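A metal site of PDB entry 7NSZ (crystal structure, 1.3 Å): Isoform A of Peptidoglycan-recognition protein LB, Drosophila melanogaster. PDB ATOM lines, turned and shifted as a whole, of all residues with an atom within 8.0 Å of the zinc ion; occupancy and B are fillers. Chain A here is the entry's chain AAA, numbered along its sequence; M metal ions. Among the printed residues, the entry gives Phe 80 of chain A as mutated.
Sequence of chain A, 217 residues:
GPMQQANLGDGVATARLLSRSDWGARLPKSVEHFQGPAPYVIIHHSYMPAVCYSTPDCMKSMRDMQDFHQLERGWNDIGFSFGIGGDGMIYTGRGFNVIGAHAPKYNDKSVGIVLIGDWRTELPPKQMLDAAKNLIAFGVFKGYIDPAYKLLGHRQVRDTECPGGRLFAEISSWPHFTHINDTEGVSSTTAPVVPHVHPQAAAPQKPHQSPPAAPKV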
ATOM      1  N   ILE A  42     -30.632 -11.571  21.902  1.00  0.00           N
ATOM      2  CA  ILE A  42     -29.735 -10.403  21.648  1.00  0.00           C
ATOM      3  C   ILE A  42     -30.551  -9.332  20.972  1.00  0.00           C
ATOM      4  O   ILE A  42     -31.164  -9.566  19.905  1.00  0.00           O
ATOM      5  CB  ILE A  42     -28.530 -10.731  20.789  1.00  0.00           C
ATOM      6  CG1 ILE A  42     -27.867 -12.045  21.162  1.00  0.00           C
ATOM      7  CG2 ILE A  42     -27.559  -9.588  20.729  1.00  0.00           C
ATOM      8  CD1 ILE A  42     -27.334 -12.102  22.504  1.00  0.00           C
ATOM      9  N   ILE A  43     -30.546  -8.143  21.529  1.00  0.00           N
ATOM     10  CA  ILE A  43     -31.267  -6.982  20.990  1.00  0.00           C
ATOM     11  C   ILE A  43     -30.364  -6.096  20.180  1.00  0.00           C
ATOM     12  O   ILE A  43     -29.223  -5.811  20.594  1.00  0.00           O
ATOM     13  CB  ILE A  43     -31.942  -6.157  22.128  1.00  0.00           C
ATOM     14  CG1 ILE A  43     -32.843  -7.023  22.989  1.00  0.00           C
ATOM     15  CG2 ILE A  43     -32.649  -4.964  21.577  1.00  0.00           C
ATOM     16  CD1 ILE A  43     -33.969  -7.709  22.270  1.00  0.00           C
ATOM     17  N   HIS A  44     -30.858  -5.659  19.038  1.00  0.00           N
ATOM     18  CA  HIS A  44     -30.200  -4.771  18.064  1.00  0.00           C
ATOM     19  C   HIS A  44     -31.092  -3.601  17.735  1.00  0.00           C
ATOM     20  O   HIS A  44     -32.342  -3.691  17.859  1.00  0.00           O
ATOM     21  CB  HIS A  44     -29.862  -5.548  16.765  1.00  0.00           C
ATOM     22  CG  HIS A  44     -29.090  -6.791  16.977  1.00  0.00           C
ATOM     23  ND1 HIS A  44     -27.704  -6.759  16.845  1.00  0.00           N
ATOM     24  CD2 HIS A  44     -29.408  -8.073  17.213  1.00  0.00           C
ATOM     25  CE1 HIS A  44     -27.227  -7.948  17.013  1.00  0.00           C
ATOM     26  NE2 HIS A  44     -28.228  -8.813  17.251  1.00  0.00           N
ATOM     27  N   HIS A  45     -30.482  -2.530  17.190  1.00  0.00           N
ATOM     28  CA  HIS A  45     -31.188  -1.540  16.369  1.00  0.00           C
ATOM     29  C   HIS A  45     -30.660  -1.673  14.943  1.00  0.00           C
ATOM     30  O   HIS A  45     -29.604  -2.273  14.708  1.00  0.00           O
ATOM     31  CB  HIS A  45     -31.152  -0.091  16.873  1.00  0.00           C
ATOM     32  CG  HIS A  45     -29.852   0.605  16.689  1.00  0.00           C
ATOM     33  ND1 HIS A  45     -29.796   1.965  16.880  1.00  0.00           N
ATOM     34  CD2 HIS A  45     -28.608   0.183  16.438  1.00  0.00           C
ATOM     35  CE1 HIS A  45     -28.553   2.344  16.709  1.00  0.00           C
ATOM     36  NE2 HIS A  45     -27.806   1.308  16.503  1.00  0.00           N
ATOM     37  N   SER A  46     -31.406  -1.129  13.996  1.00  0.00           N
ATOM     38  CA  SER A  46     -30.941  -1.218  12.596  1.00  0.00           C
ATOM     39  C   SER A  46     -30.015  -0.056  12.244  1.00  0.00           C
ATOM     40  O   SER A  46     -29.147  -0.239  11.369  1.00  0.00           O
ATOM     41  CB  SER A  46     -32.088  -1.280  11.601  1.00  0.00           C
ATOM     42  OG  SER A  46     -32.921  -0.129  11.665  1.00  0.00           O
ATOM     43  N   PHE A  80     -30.739 -11.112  11.059  1.00  0.00           N
ATOM     44  CA  PHE A  80     -31.545 -11.149  12.291  1.00  0.00           C
ATOM     45  C   PHE A  80     -32.563 -12.278  12.255  1.00  0.00           C
ATOM     46  O   PHE A  80     -33.104 -12.656  11.187  1.00  0.00           O
ATOM     47  CB  PHE A  80     -32.244  -9.791  12.449  1.00  0.00           C
ATOM     48  CG  PHE A  80     -31.293  -8.633  12.467  1.00  0.00           C
ATOM     49  CD1 PHE A  80     -30.388  -8.465  13.522  1.00  0.00           C
ATOM     50  CD2 PHE A  80     -31.301  -7.684  11.468  1.00  0.00           C
ATOM     51  CE1 PHE A  80     -29.499  -7.401  13.554  1.00  0.00           C
ATOM     52  CE2 PHE A  80     -30.435  -6.616  11.506  1.00  0.00           C
ATOM     53  CZ  PHE A  80     -29.498  -6.492  12.540  1.00  0.00           C
ATOM     54  N   HIS A 102     -25.822 -12.110  13.239  1.00  0.00           N
ATOM     55  CA  HIS A 102     -26.031 -10.834  13.963  1.00  0.00           C
ATOM     56  C   HIS A 102     -25.102 -10.687  15.167  1.00  0.00           C
ATOM     57  O   HIS A 102     -24.962  -9.554  15.588  1.00  0.00           O
ATOM     58  CB  HIS A 102     -27.519 -10.664  14.352  1.00  0.00           C
ATOM     59  CG  HIS A 102     -28.004 -11.689  15.318  1.00  0.00           C
ATOM     60  ND1 HIS A 102     -27.887 -11.583  16.691  1.00  0.00           N
ATOM     61  CD2 HIS A 102     -28.504 -12.926  15.091  1.00  0.00           C
ATOM     62  CE1 HIS A 102     -28.278 -12.722  17.233  1.00  0.00           C
ATOM     63  NE2 HIS A 102     -28.636 -13.606  16.248  1.00  0.00           N
ATOM     64  N   ALA A 103     -24.622 -11.742  15.766  1.00  0.00           N
ATOM     65  CA  ALA A 103     -23.857 -11.610  17.024  1.00  0.00           C
ATOM     66  C   ALA A 103     -22.824 -12.721  17.060  1.00  0.00           C
ATOM     67  O   ALA A 103     -23.124 -13.835  17.409  1.00  0.00           O
ATOM     68  CB  ALA A 103     -24.791 -11.702  18.203  1.00  0.00           C
ATOM     69  N   ILE A 113     -33.008  -9.984  17.655  1.00  0.00           N
ATOM     70  CA  ILE A 113     -34.205  -9.185  17.391  1.00  0.00           C
ATOM     71  C   ILE A 113     -33.763  -7.780  17.061  1.00  0.00           C
ATOM     72  O   ILE A 113     -33.068  -7.190  17.921  1.00  0.00           O
ATOM     73  CB  ILE A 113     -35.172  -9.177  18.594  1.00  0.00           C
ATOM     74  CG1 ILE A 113     -35.586 -10.592  18.996  1.00  0.00           C
ATOM     75  CG2 ILE A 113     -36.386  -8.294  18.319  1.00  0.00           C
ATOM     76  CD1 ILE A 113     -36.334 -10.657  20.365  1.00  0.00           C
ATOM     77  N   VAL A 114     -34.066  -7.273  15.892  1.00  0.00           N
ATOM     78  CA  VAL A 114     -33.732  -5.876  15.527  1.00  0.00           C
ATOM     79  C   VAL A 114     -34.979  -5.026  15.674  1.00  0.00           C
ATOM     80  O   VAL A 114     -36.042  -5.290  15.123  1.00  0.00           O
ATOM     81  CB  VAL A 114     -33.110  -5.787  14.116  1.00  0.00           C
ATOM     82  CG1 VAL A 114     -34.040  -6.204  13.007  1.00  0.00           C
ATOM     83  CG2 VAL A 114     -32.582  -4.380  13.876  1.00  0.00           C
ATOM     84  N   GLY A 153     -27.722  -6.844  24.972  1.00  0.00           N
ATOM     85  CA  GLY A 153     -27.566  -6.028  23.780  1.00  0.00           C
ATOM     86  C   GLY A 153     -26.320  -6.437  23.033  1.00  0.00           C
ATOM     87  O   GLY A 153     -25.365  -6.970  23.596  1.00  0.00           O
ATOM     88  N   HIS A 154     -26.332  -6.197  21.744  1.00  0.00           N
ATOM     89  CA  HIS A 154     -25.165  -6.490  20.883  1.00  0.00           C
ATOM     90  C   HIS A 154     -23.858  -5.927  21.446  1.00  0.00           C
ATOM     91  O   HIS A 154     -22.873  -6.648  21.416  1.00  0.00           O
ATOM     92  CB  HIS A 154     -25.478  -5.958  19.509  1.00  0.00           C
ATOM     93  CG  HIS A 154     -24.566  -6.364  18.394  1.00  0.00           C
ATOM     94  ND1 HIS A 154     -24.745  -5.922  17.124  1.00  0.00           N
ATOM     95  CD2 HIS A 154     -23.396  -7.038  18.370  1.00  0.00           C
ATOM     96  CE1 HIS A 154     -23.759  -6.357  16.360  1.00  0.00           C
ATOM     97  NE2 HIS A 154     -22.949  -7.076  17.070  1.00  0.00           N
ATOM     98  N   ARG A 155     -23.907  -4.722  22.000  1.00  0.00           N
ATOM     99  CA  ARG A 155     -22.684  -4.039  22.513  1.00  0.00           C
ATOM    100  C   ARG A 155     -22.064  -4.867  23.633  1.00  0.00           C
ATOM    101  O   ARG A 155     -20.890  -4.565  23.944  1.00  0.00           O
ATOM    102  CB  ARG A 155     -23.046  -2.638  22.984  1.00  0.00           C
ATOM    103  CG  ARG A 155     -24.056  -2.593  24.100  1.00  0.00           C
ATOM    104  CD  ARG A 155     -24.106  -1.255  24.850  1.00  0.00           C
ATOM    105  NE  ARG A 155     -24.469  -0.203  23.925  1.00  0.00           N
ATOM    106  CZ  ARG A 155     -24.460   1.101  24.224  1.00  0.00           C
ATOM    107  NH1 ARG A 155     -24.214   1.462  25.466  1.00  0.00           N
ATOM    108  NH2 ARG A 155     -24.742   2.003  23.320  1.00  0.00           N
ATOM    109  N   ARG A 158     -19.661  -7.494  21.426  1.00  0.00           N
ATOM    110  CA  ARG A 158     -18.773  -7.023  20.344  1.00  0.00           C
ATOM    111  C   ARG A 158     -18.583  -5.554  20.497  1.00  0.00           C
ATOM    112  O   ARG A 158     -19.327  -4.841  21.194  1.00  0.00           O
ATOM    113  CB  ARG A 158     -19.370  -7.275  18.950  1.00  0.00           C
ATOM    114  CG  ARG A 158     -19.307  -8.727  18.515  1.00  0.00           C
ATOM    115  CD  ARG A 158     -17.910  -9.219  18.342  1.00  0.00           C
ATOM    116  NE  ARG A 158     -17.092  -8.357  17.518  1.00  0.00           N
ATOM    117  CZ  ARG A 158     -15.777  -8.407  17.470  1.00  0.00           C
ATOM    118  NH1 ARG A 158     -15.135  -9.343  18.168  1.00  0.00           N
ATOM    119  NH2 ARG A 158     -15.136  -7.521  16.742  1.00  0.00           N
ATOM    120  N   THR A 160     -19.378  -2.538  19.479  1.00  0.00           N
ATOM    121  CA  THR A 160     -20.419  -1.823  18.711  1.00  0.00           C
ATOM    122  C   THR A 160     -21.215  -0.954  19.681  1.00  0.00           C
ATOM    123  O   THR A 160     -21.259  -1.326  20.855  1.00  0.00           O
ATOM    124  CB  THR A 160     -21.404  -2.798  18.032  1.00  0.00           C
ATOM    125  OG1 THR A 160     -22.316  -2.027  17.289  1.00  0.00           O
ATOM    126  CG2 THR A 160     -22.217  -3.668  18.962  1.00  0.00           C
ATOM    127  N   GLU A 161     -21.833   0.090  19.194  1.00  0.00           N
ATOM    128  CA  GLU A 161     -22.821   0.946  19.874  1.00  0.00           C
ATOM    129  C   GLU A 161     -24.225   0.304  19.926  1.00  0.00           C
ATOM    130  O   GLU A 161     -25.013   0.634  20.811  1.00  0.00           O
ATOM    131  CB  GLU A 161     -22.874   2.236  19.063  1.00  0.00           C
ATOM    132  CG  GLU A 161     -23.767   3.318  19.602  1.00  0.00           C
ATOM    133  CD  GLU A 161     -23.358   4.692  19.099  1.00  0.00           C
ATOM    134  OE1 GLU A 161     -23.864   5.699  19.616  1.00  0.00           O
ATOM    135  OE2 GLU A 161     -22.529   4.763  18.160  1.00  0.00           O
ATOM    136  N   CYS A 162     -24.498  -0.555  18.954  1.00  0.00           N
ATOM    137  CA  CYS A 162     -25.804  -1.274  18.867  1.00  0.00           C
ATOM    138  C   CYS A 162     -26.140  -1.879  20.234  1.00  0.00           C
ATOM    139  O   CYS A 162     -25.330  -2.567  20.846  1.00  0.00           O
ATOM    140  CB  CYS A 162     -25.697  -2.337  17.784  1.00  0.00           C
ATOM    141  SG  CYS A 162     -27.234  -3.241  17.597  1.00  0.00           S
ATOM    142  N   PRO A 163     -27.400  -1.757  20.742  1.00  0.00           N
ATOM    143  CA  PRO A 163     -28.592  -1.228  20.065  1.00  0.00           C
ATOM    144  C   PRO A 163     -28.940   0.247  20.263  1.00  0.00           C
ATOM    145  O   PRO A 163     -30.050   0.642  20.131  1.00  0.00           O
ATOM    146  CB  PRO A 163     -29.703  -2.097  20.707  1.00  0.00           C
ATOM    147  CG  PRO A 163     -29.231  -2.243  22.170  1.00  0.00           C
ATOM    148  CD  PRO A 163     -27.747  -2.470  21.998  1.00  0.00           C
ATOM    149  N   GLY A 164     -27.888   1.053  20.494  1.00  0.00           N
ATOM    150  CA  GLY A 164     -28.043   2.487  20.837  1.00  0.00           C
ATOM    151  C   GLY A 164     -28.119   2.643  22.334  1.00  0.00           C
ATOM    152  O   GLY A 164     -28.701   1.836  23.004  1.00  0.00           O
HETATM  153 ZN    ZN M   1     -26.526  -5.094  16.485  1.00  0.00          ZN
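The zinc ion is bound by ND1 of His 154, 2.1 Å away.
The zinc ion is bound by ND1 of His 44, at 2.1 Å.
SG of Cys 162 is bound to the zinc ion (2.3 Å).
Of the 19 residues printed, 3 come within 4 Å of the zinc ion.
The backbone carbonyl oxygen (O) of Ile 43 sits at hydrogen-bond distance from the backbone NH (N) of His 154, at 3.1 Å.
A ring nitrogen (NE2) of His 44 sits at hydrogen-bond distance from a ring nitrogen (ND1) of His 102 (2.8 Å).
The backbone NH (N) of His 44 lies within hydrogen-bond range of the backbone carbonyl oxygen (O) of Ile 113 (2.9 Å).
SG of Cys 162 lies close to N of His 45 (3.3 Å).
OG1 of Thr 160 lies within hydrogen-bond range of N of Cys 162.
N of Arg 155 lies within hydrogen-bond range of O of Cys 162 (2.8 Å).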
